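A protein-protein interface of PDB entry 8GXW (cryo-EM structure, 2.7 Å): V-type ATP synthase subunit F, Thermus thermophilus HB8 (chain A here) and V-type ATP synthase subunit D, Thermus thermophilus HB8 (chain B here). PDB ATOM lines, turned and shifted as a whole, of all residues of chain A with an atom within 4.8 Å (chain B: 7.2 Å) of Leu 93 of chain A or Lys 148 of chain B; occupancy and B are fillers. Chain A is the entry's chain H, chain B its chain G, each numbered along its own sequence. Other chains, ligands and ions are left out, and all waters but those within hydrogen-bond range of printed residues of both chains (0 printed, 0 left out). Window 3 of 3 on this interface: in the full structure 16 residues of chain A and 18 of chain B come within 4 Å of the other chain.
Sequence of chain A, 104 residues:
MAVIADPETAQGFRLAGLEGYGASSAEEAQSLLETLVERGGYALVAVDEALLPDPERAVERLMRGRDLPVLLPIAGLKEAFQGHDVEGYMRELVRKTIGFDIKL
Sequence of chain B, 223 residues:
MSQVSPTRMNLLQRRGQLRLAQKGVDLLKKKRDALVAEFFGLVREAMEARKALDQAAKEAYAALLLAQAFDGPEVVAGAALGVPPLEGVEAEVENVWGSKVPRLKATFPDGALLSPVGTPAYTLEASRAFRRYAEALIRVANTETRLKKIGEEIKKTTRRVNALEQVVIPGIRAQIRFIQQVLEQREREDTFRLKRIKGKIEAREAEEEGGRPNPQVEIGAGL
The side-chain hydroxyl of Tyr 89 of chain A is in hydrogen-bond range of the guanidinium group of Arg 50 of chain B (3.1 Å).
OE2 of Glu 144 of chain B is in hydrogen-bond range of OH of Tyr 89 of chain A (3.4 Å).
Of the printed residues of chain B, Leu 93 of chain A touches Leu 147 (3.2 Å) and Lys 148 (3.6 Å).
Lys 148 of chain B touches just one residue of chain A: Leu 93 (3.6 Å).
Of the printed residues of chain A, Leu 147 of chain B touches Leu 93 (3.2 Å).
Of the printed residues of chain B, Tyr 89 of chain A touches Arg 50 and Glu 144.
Printed residues of chain A within 4 Å of Glu 144 of chain B: Tyr 89 (3.4 Å).
Ala 46 of chain B touches none of the printed residues of chain A.
Arg 146 of chain B touches none of the printed residues of chain A.
The nearest residue of chain B that does not touch Leu 93 of chain A is Glu 144 of chain B (5.5 Å).
The nearest printed residue of chain A that does not touch Lys 148 of chain B is Tyr 89 of chain A (5.0 Å).
NH2 of Arg 50 of chain B lies within salt-bridge range of OE1 of Glu 144 of chain B (3.97 Å).
The side-chain amino group (NZ) of Lys 148 of chain B is in hydrogen-bond range of the backbone carbonyl oxygen (O) of Glu 144 of chain B.
CD2 of Leu 147 of chain B touches CD2 of Leu 93 of chain A, at 3.2 Å.
CD1 of Leu 93 of chain A touches CE of Lys 148 of chain B (3.6 Å).
Thr 97 of chain A touches Phe 39 of chain B.
Gly 151 of chain B touches Thr 97 of chain A (CA to OG1, 3.4 Å).
Hydrophobic or aromatic side chains of chain A within 4 Å of the printed part of chain B: Tyr 89 and Leu 93.
Along chain A the printed residues that touch a printed residue of chain B span positions 89 to 97.
Printed residues of chain B that touch a printed residue of chain A: Phe 39, Arg 50, Glu 144, Leu 147, Lys 148 and Gly 151.
Hydrophobic or aromatic side chains of chain B that line the printed part of chain A: Phe 39 and Leu 147.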
ATOM      1  N   GLY A  88     -10.573  -0.817  38.753  1.00  0.00           N
ATOM      2  CA  GLY A  88     -10.913   0.265  37.854  1.00  0.00           C
ATOM      3  C   GLY A  88      -9.754   0.673  36.972  1.00  0.00           C
ATOM      4  O   GLY A  88      -9.950   1.041  35.812  1.00  0.00           O
ATOM      5  N   TYR A  89      -8.532   0.610  37.496  1.00  0.00           N
ATOM      6  CA  TYR A  89      -7.384   1.032  36.707  1.00  0.00           C
ATOM      7  C   TYR A  89      -7.244   0.172  35.460  1.00  0.00           C
ATOM      8  O   TYR A  89      -7.186   0.688  34.338  1.00  0.00           O
ATOM      9  CB  TYR A  89      -6.115   0.970  37.554  1.00  0.00           C
ATOM     10  CG  TYR A  89      -4.858   0.777  36.742  1.00  0.00           C
ATOM     11  CD1 TYR A  89      -4.473   1.714  35.795  1.00  0.00           C
ATOM     12  CD2 TYR A  89      -4.061  -0.345  36.917  1.00  0.00           C
ATOM     13  CE1 TYR A  89      -3.330   1.544  35.050  1.00  0.00           C
ATOM     14  CE2 TYR A  89      -2.913  -0.524  36.173  1.00  0.00           C
ATOM     15  CZ  TYR A  89      -2.552   0.425  35.240  1.00  0.00           C
ATOM     16  OH  TYR A  89      -1.408   0.251  34.496  1.00  0.00           O
ATOM     17  N   MET A  90      -7.221  -1.151  35.634  1.00  0.00           N
ATOM     18  CA  MET A  90      -7.092  -2.042  34.486  1.00  0.00           C
ATOM     19  C   MET A  90      -8.345  -2.032  33.620  1.00  0.00           C
ATOM     20  O   MET A  90      -8.249  -2.168  32.398  1.00  0.00           O
ATOM     21  CB  MET A  90      -6.787  -3.461  34.957  1.00  0.00           C
ATOM     22  CG  MET A  90      -7.928  -4.109  35.728  1.00  0.00           C
ATOM     23  SD  MET A  90      -7.416  -5.398  36.880  1.00  0.00           S
ATOM     24  CE  MET A  90      -6.166  -4.559  37.850  1.00  0.00           C
ATOM     25  N   ARG A  91      -9.524  -1.883  34.226  1.00  0.00           N
ATOM     26  CA  ARG A  91     -10.741  -1.753  33.431  1.00  0.00           C
ATOM     27  C   ARG A  91     -10.635  -0.580  32.469  1.00  0.00           C
ATOM     28  O   ARG A  91     -10.847  -0.726  31.260  1.00  0.00           O
ATOM     29  CB  ARG A  91     -11.947  -1.575  34.351  1.00  0.00           C
ATOM     30  CG  ARG A  91     -12.527  -2.862  34.894  1.00  0.00           C
ATOM     31  CD  ARG A  91     -13.393  -3.561  33.859  1.00  0.00           C
ATOM     32  NE  ARG A  91     -14.198  -4.625  34.447  1.00  0.00           N
ATOM     33  CZ  ARG A  91     -15.416  -4.461  34.947  1.00  0.00           C
ATOM     34  NH1 ARG A  91     -16.007  -3.276  34.958  1.00  0.00           N
ATOM     35  NH2 ARG A  91     -16.057  -5.511  35.451  1.00  0.00           N
ATOM     36  N   GLU A  92     -10.303   0.600  32.994  1.00  0.00           N
ATOM     37  CA  GLU A  92     -10.152   1.772  32.144  1.00  0.00           C
ATOM     38  C   GLU A  92      -9.006   1.594  31.163  1.00  0.00           C
ATOM     39  O   GLU A  92      -9.066   2.105  30.039  1.00  0.00           O
ATOM     40  CB  GLU A  92      -9.935   3.015  33.005  1.00  0.00           C
ATOM     41  CG  GLU A  92     -10.093   4.332  32.256  1.00  0.00           C
ATOM     42  CD  GLU A  92      -8.788   4.847  31.676  1.00  0.00           C
ATOM     43  OE1 GLU A  92      -7.713   4.501  32.209  1.00  0.00           O
ATOM     44  OE2 GLU A  92      -8.839   5.602  30.682  1.00  0.00           O
ATOM     45  N   LEU A  93      -7.959   0.875  31.559  1.00  0.00           N
ATOM     46  CA  LEU A  93      -6.853   0.632  30.645  1.00  0.00           C
ATOM     47  C   LEU A  93      -7.316  -0.170  29.435  1.00  0.00           C
ATOM     48  O   LEU A  93      -6.968   0.146  28.290  1.00  0.00           O
ATOM     49  CB  LEU A  93      -5.729  -0.087  31.388  1.00  0.00           C
ATOM     50  CG  LEU A  93      -4.524  -0.533  30.563  1.00  0.00           C
ATOM     51  CD1 LEU A  93      -3.872   0.635  29.841  1.00  0.00           C
ATOM     52  CD2 LEU A  93      -3.524  -1.221  31.475  1.00  0.00           C
ATOM     53  N   VAL A  94      -8.108  -1.214  29.674  1.00  0.00           N
ATOM     54  CA  VAL A  94      -8.686  -1.973  28.572  1.00  0.00           C
ATOM     55  C   VAL A  94      -9.590  -1.080  27.743  1.00  0.00           C
ATOM     56  O   VAL A  94      -9.559  -1.110  26.508  1.00  0.00           O
ATOM     57  CB  VAL A  94      -9.446  -3.201  29.102  1.00  0.00           C
ATOM     58  CG1 VAL A  94     -10.169  -3.901  27.969  1.00  0.00           C
ATOM     59  CG2 VAL A  94      -8.489  -4.153  29.789  1.00  0.00           C
ATOM     60  N   ARG A  95     -10.419  -0.278  28.406  1.00  0.00           N
ATOM     61  CA  ARG A  95     -11.260   0.656  27.671  1.00  0.00           C
ATOM     62  C   ARG A  95     -10.414   1.493  26.723  1.00  0.00           C
ATOM     63  O   ARG A  95     -10.816   1.767  25.587  1.00  0.00           O
ATOM     64  CB  ARG A  95     -12.033   1.547  28.648  1.00  0.00           C
ATOM     65  CG  ARG A  95     -13.018   2.513  27.991  1.00  0.00           C
ATOM     66  CD  ARG A  95     -13.464   3.613  28.951  1.00  0.00           C
ATOM     67  NE  ARG A  95     -14.195   3.083  30.098  1.00  0.00           N
ATOM     68  CZ  ARG A  95     -14.182   3.611  31.317  1.00  0.00           C
ATOM     69  NH1 ARG A  95     -13.489   4.706  31.592  1.00  0.00           N
ATOM     70  NH2 ARG A  95     -14.886   3.029  32.282  1.00  0.00           N
ATOM     71  N   LYS A  96      -9.220   1.884  27.166  1.00  0.00           N
ATOM     72  CA  LYS A  96      -8.378   2.743  26.345  1.00  0.00           C
ATOM     73  C   LYS A  96      -7.759   1.977  25.183  1.00  0.00           C
ATOM     74  O   LYS A  96      -7.720   2.481  24.054  1.00  0.00           O
ATOM     75  CB  LYS A  96      -7.288   3.381  27.206  1.00  0.00           C
ATOM     76  CG  LYS A  96      -7.791   4.478  28.140  1.00  0.00           C
ATOM     77  CD  LYS A  96      -8.162   5.755  27.393  1.00  0.00           C
ATOM     78  CE  LYS A  96      -6.936   6.586  27.051  1.00  0.00           C
ATOM     79  NZ  LYS A  96      -6.293   7.160  28.266  1.00  0.00           N
ATOM     80  N   THR A  97      -7.275   0.760  25.429  1.00  0.00           N
ATOM     81  CA  THR A  97      -6.493   0.064  24.407  1.00  0.00           C
ATOM     82  C   THR A  97      -7.340  -0.741  23.426  1.00  0.00           C
ATOM     83  O   THR A  97      -6.945  -0.880  22.263  1.00  0.00           O
ATOM     84  CB  THR A  97      -5.457  -0.866  25.050  1.00  0.00           C
ATOM     85  OG1 THR A  97      -4.758  -1.578  24.022  1.00  0.00           O
ATOM     86  CG2 THR A  97      -6.107  -1.860  25.990  1.00  0.00           C
ATOM     87  N   PHE B  39      -3.266 -11.643  25.374  1.00  0.00           N
ATOM     88  CA  PHE B  39      -3.495 -10.376  26.057  1.00  0.00           C
ATOM     89  C   PHE B  39      -4.388 -10.561  27.274  1.00  0.00           C
ATOM     90  O   PHE B  39      -4.161  -9.947  28.321  1.00  0.00           O
ATOM     91  CB  PHE B  39      -4.104  -9.385  25.069  1.00  0.00           C
ATOM     92  CG  PHE B  39      -4.547  -8.098  25.679  1.00  0.00           C
ATOM     93  CD1 PHE B  39      -5.830  -7.954  26.159  1.00  0.00           C
ATOM     94  CD2 PHE B  39      -3.695  -7.021  25.738  1.00  0.00           C
ATOM     95  CE1 PHE B  39      -6.242  -6.771  26.707  1.00  0.00           C
ATOM     96  CE2 PHE B  39      -4.106  -5.835  26.285  1.00  0.00           C
ATOM     97  CZ  PHE B  39      -5.382  -5.711  26.769  1.00  0.00           C
ATOM     98  N   LEU B  42      -2.198 -12.020  29.979  1.00  0.00           N
ATOM     99  CA  LEU B  42      -1.197 -11.072  30.427  1.00  0.00           C
ATOM    100  C   LEU B  42      -1.830  -9.970  31.262  1.00  0.00           C
ATOM    101  O   LEU B  42      -1.173  -9.409  32.142  1.00  0.00           O
ATOM    102  CB  LEU B  42      -0.456 -10.499  29.223  1.00  0.00           C
ATOM    103  CG  LEU B  42       0.677  -9.531  29.539  1.00  0.00           C
ATOM    104  CD1 LEU B  42       1.750  -9.658  28.497  1.00  0.00           C
ATOM    105  CD2 LEU B  42       0.198  -8.100  29.594  1.00  0.00           C
ATOM    106  N   VAL B  43      -3.104  -9.663  31.027  1.00  0.00           N
ATOM    107  CA  VAL B  43      -3.798  -8.724  31.902  1.00  0.00           C
ATOM    108  C   VAL B  43      -3.963  -9.320  33.294  1.00  0.00           C
ATOM    109  O   VAL B  43      -3.854  -8.613  34.303  1.00  0.00           O
ATOM    110  CB  VAL B  43      -5.155  -8.323  31.299  1.00  0.00           C
ATOM    111  CG1 VAL B  43      -6.096  -9.511  31.270  1.00  0.00           C
ATOM    112  CG2 VAL B  43      -5.758  -7.194  32.096  1.00  0.00           C
ATOM    113  N   ALA B  46      -0.723  -8.908  34.940  1.00  0.00           N
ATOM    114  CA  ALA B  46      -0.491  -7.516  35.299  1.00  0.00           C
ATOM    115  C   ALA B  46      -1.269  -7.134  36.546  1.00  0.00           C
ATOM    116  O   ALA B  46      -0.753  -6.423  37.410  1.00  0.00           O
ATOM    117  CB  ALA B  46      -0.869  -6.603  34.134  1.00  0.00           C
ATOM    118  N   ARG B  50       0.126  -5.910  40.081  1.00  0.00           N
ATOM    119  CA  ARG B  50      -0.266  -4.615  40.622  1.00  0.00           C
ATOM    120  C   ARG B  50      -0.745  -4.736  42.061  1.00  0.00           C
ATOM    121  O   ARG B  50      -0.392  -3.907  42.908  1.00  0.00           O
ATOM    122  CB  ARG B  50      -1.350  -3.991  39.746  1.00  0.00           C
ATOM    123  CG  ARG B  50      -1.893  -2.670  40.262  1.00  0.00           C
ATOM    124  CD  ARG B  50      -0.797  -1.628  40.402  1.00  0.00           C
ATOM    125  NE  ARG B  50      -0.188  -1.297  39.118  1.00  0.00           N
ATOM    126  CZ  ARG B  50      -0.516  -0.250  38.373  1.00  0.00           C
ATOM    127  NH1 ARG B  50      -1.466   0.595  38.740  1.00  0.00           N
ATOM    128  NH2 ARG B  50       0.127  -0.044  37.228  1.00  0.00           N
ATOM    129  N   THR B 143       5.571  -5.655  33.231  1.00  0.00           N
ATOM    130  CA  THR B 143       4.324  -6.194  32.695  1.00  0.00           C
ATOM    131  C   THR B 143       3.546  -5.130  31.924  1.00  0.00           C
ATOM    132  O   THR B 143       2.943  -5.426  30.882  1.00  0.00           O
ATOM    133  CB  THR B 143       3.462  -6.787  33.811  1.00  0.00           C
ATOM    134  OG1 THR B 143       2.224  -7.254  33.261  1.00  0.00           O
ATOM    135  CG2 THR B 143       3.173  -5.763  34.892  1.00  0.00           C
ATOM    136  N   GLU B 144       3.559  -3.885  32.405  1.00  0.00           N
ATOM    137  CA  GLU B 144       2.760  -2.842  31.771  1.00  0.00           C
ATOM    138  C   GLU B 144       3.269  -2.518  30.373  1.00  0.00           C
ATOM    139  O   GLU B 144       2.474  -2.310  29.448  1.00  0.00           O
ATOM    140  CB  GLU B 144       2.759  -1.588  32.644  1.00  0.00           C
ATOM    141  CG  GLU B 144       1.880  -0.467  32.118  1.00  0.00           C
ATOM    142  CD  GLU B 144       1.823   0.719  33.059  1.00  0.00           C
ATOM    143  OE1 GLU B 144       2.488   0.671  34.114  1.00  0.00           O
ATOM    144  OE2 GLU B 144       1.112   1.696  32.744  1.00  0.00           O
ATOM    145  N   THR B 145       4.588  -2.461  30.198  1.00  0.00           N
ATOM    146  CA  THR B 145       5.128  -2.169  28.874  1.00  0.00           C
ATOM    147  C   THR B 145       4.712  -3.232  27.866  1.00  0.00           C
ATOM    148  O   THR B 145       4.313  -2.914  26.737  1.00  0.00           O
ATOM    149  CB  THR B 145       6.649  -2.064  28.934  1.00  0.00           C
ATOM    150  OG1 THR B 145       7.191  -3.264  29.497  1.00  0.00           O
ATOM    151  CG2 THR B 145       7.075  -0.866  29.772  1.00  0.00           C
ATOM    152  N   ARG B 146       4.786  -4.504  28.256  1.00  0.00           N
ATOM    153  CA  ARG B 146       4.412  -5.562  27.330  1.00  0.00           C
ATOM    154  C   ARG B 146       2.916  -5.544  27.052  1.00  0.00           C
ATOM    155  O   ARG B 146       2.491  -5.851  25.933  1.00  0.00           O
ATOM    156  CB  ARG B 146       4.842  -6.916  27.880  1.00  0.00           C
ATOM    157  CG  ARG B 146       4.387  -8.094  27.034  1.00  0.00           C
ATOM    158  CD  ARG B 146       5.008  -9.417  27.474  1.00  0.00           C
ATOM    159  NE  ARG B 146       6.313  -9.260  28.102  1.00  0.00           N
ATOM    160  CZ  ARG B 146       6.510  -9.084  29.403  1.00  0.00           C
ATOM    161  NH1 ARG B 146       5.499  -9.025  30.255  1.00  0.00           N
ATOM    162  NH2 ARG B 146       7.753  -8.960  29.859  1.00  0.00           N
ATOM    163  N   LEU B 147       2.105  -5.187  28.049  1.00  0.00           N
ATOM    164  CA  LEU B 147       0.678  -5.033  27.798  1.00  0.00           C
ATOM    165  C   LEU B 147       0.427  -3.950  26.753  1.00  0.00           C
ATOM    166  O   LEU B 147      -0.385  -4.130  25.837  1.00  0.00           O
ATOM    167  CB  LEU B 147      -0.050  -4.707  29.099  1.00  0.00           C
ATOM    168  CG  LEU B 147      -1.582  -4.700  29.019  1.00  0.00           C
ATOM    169  CD1 LEU B 147      -2.182  -6.011  29.497  1.00  0.00           C
ATOM    170  CD2 LEU B 147      -2.155  -3.538  29.806  1.00  0.00           C
ATOM    171  N   LYS B 148       1.118  -2.813  26.876  1.00  0.00           N
ATOM    172  CA  LYS B 148       0.963  -1.759  25.876  1.00  0.00           C
ATOM    173  C   LYS B 148       1.360  -2.265  24.500  1.00  0.00           C
ATOM    174  O   LYS B 148       0.693  -1.971  23.497  1.00  0.00           O
ATOM    175  CB  LYS B 148       1.822  -0.542  26.230  1.00  0.00           C
ATOM    176  CG  LYS B 148       1.531   0.153  27.556  1.00  0.00           C
ATOM    177  CD  LYS B 148       0.073   0.525  27.767  1.00  0.00           C
ATOM    178  CE  LYS B 148      -0.282   0.457  29.240  1.00  0.00           C
ATOM    179  NZ  LYS B 148      -0.185  -0.931  29.764  1.00  0.00           N
ATOM    180  N   LYS B 149       2.460  -3.015  24.432  1.00  0.00           N
ATOM    181  CA  LYS B 149       2.926  -3.534  23.152  1.00  0.00           C
ATOM    182  C   LYS B 149       1.879  -4.440  22.518  1.00  0.00           C
ATOM    183  O   LYS B 149       1.587  -4.329  21.323  1.00  0.00           O
ATOM    184  CB  LYS B 149       4.244  -4.281  23.346  1.00  0.00           C
ATOM    185  CG  LYS B 149       4.845  -4.852  22.063  1.00  0.00           C
ATOM    186  CD  LYS B 149       5.274  -3.763  21.085  1.00  0.00           C
ATOM    187  CE  LYS B 149       6.468  -2.973  21.601  1.00  0.00           C
ATOM    188  NZ  LYS B 149       6.995  -2.022  20.584  1.00  0.00           N
ATOM    189  N   ILE B 150       1.300  -5.349  23.298  1.00  0.00           N
ATOM    190  CA  ILE B 150       0.310  -6.253  22.728  1.00  0.00           C
ATOM    191  C   ILE B 150      -0.932  -5.483  22.309  1.00  0.00           C
ATOM    192  O   ILE B 150      -1.573  -5.813  21.304  1.00  0.00           O
ATOM    193  CB  ILE B 150      -0.040  -7.383  23.709  1.00  0.00           C
ATOM    194  CG1 ILE B 150       1.191  -8.236  24.018  1.00  0.00           C
ATOM    195  CG2 ILE B 150      -1.149  -8.241  23.135  1.00  0.00           C
ATOM    196  CD1 ILE B 150       1.918  -8.740  22.805  1.00  0.00           C
ATOM    197  N   GLY B 151      -1.307  -4.462  23.072  1.00  0.00           N
ATOM    198  CA  GLY B 151      -2.439  -3.648  22.668  1.00  0.00           C
ATOM    199  C   GLY B 151      -2.209  -2.998  21.319  1.00  0.00           C
ATOM    200  O   GLY B 151      -3.081  -3.014  20.446  1.00  0.00           O
ATOM    201  N   GLU B 152      -1.023  -2.427  21.130  1.00  0.00           N
ATOM    202  CA  GLU B 152      -0.719  -1.803  19.849  1.00  0.00           C
ATOM    203  C   GLU B 152      -0.660  -2.837  18.733  1.00  0.00           C
ATOM    204  O   GLU B 152      -1.069  -2.552  17.604  1.00  0.00           O
ATOM    205  CB  GLU B 152       0.591  -1.014  19.942  1.00  0.00           C
ATOM    206  CG  GLU B 152       1.839  -1.732  19.437  1.00  0.00           C
ATOM    207  CD  GLU B 152       3.063  -0.837  19.448  1.00  0.00           C
ATOM    208  OE1 GLU B 152       2.907   0.387  19.643  1.00  0.00           O
ATOM    209  OE2 GLU B 152       4.183  -1.357  19.260  1.00  0.00           O
ATOM    210  N   GLU B 153      -0.165  -4.041  19.025  1.00  0.00           N
ATOM    211  CA  GLU B 153      -0.152  -5.094  18.011  1.00  0.00           C
ATOM    212  C   GLU B 153      -1.564  -5.475  17.589  1.00  0.00           C
ATOM    213  O   GLU B 153      -1.837  -5.653  16.397  1.00  0.00           O
ATOM    214  CB  GLU B 153       0.596  -6.317  18.535  1.00  0.00           C
ATOM    215  CG  GLU B 153       2.093  -6.108  18.687  1.00  0.00           C
ATOM    216  CD  GLU B 153       2.787  -7.293  19.332  1.00  0.00           C
ATOM    217  OE1 GLU B 153       2.082  -8.201  19.823  1.00  0.00           O
ATOM    218  OE2 GLU B 153       4.035  -7.316  19.348  1.00  0.00           O
ATOM    219  N   ILE B 154      -2.477  -5.604  18.551  1.00  0.00           N
ATOM    220  CA  ILE B 154      -3.859  -5.945  18.221  1.00  0.00           C
ATOM    221  C   ILE B 154      -4.498  -4.825  17.413  1.00  0.00           C
ATOM    222  O   ILE B 154      -5.227  -5.071  16.443  1.00  0.00           O
ATOM    223  CB  ILE B 154      -4.651  -6.247  19.506  1.00  0.00           C
ATOM    224  CG1 ILE B 154      -4.144  -7.538  20.144  1.00  0.00           C
ATOM    225  CG2 ILE B 154      -6.132  -6.364  19.215  1.00  0.00           C
ATOM    226  CD1 ILE B 154      -4.507  -7.679  21.607  1.00  0.00           C
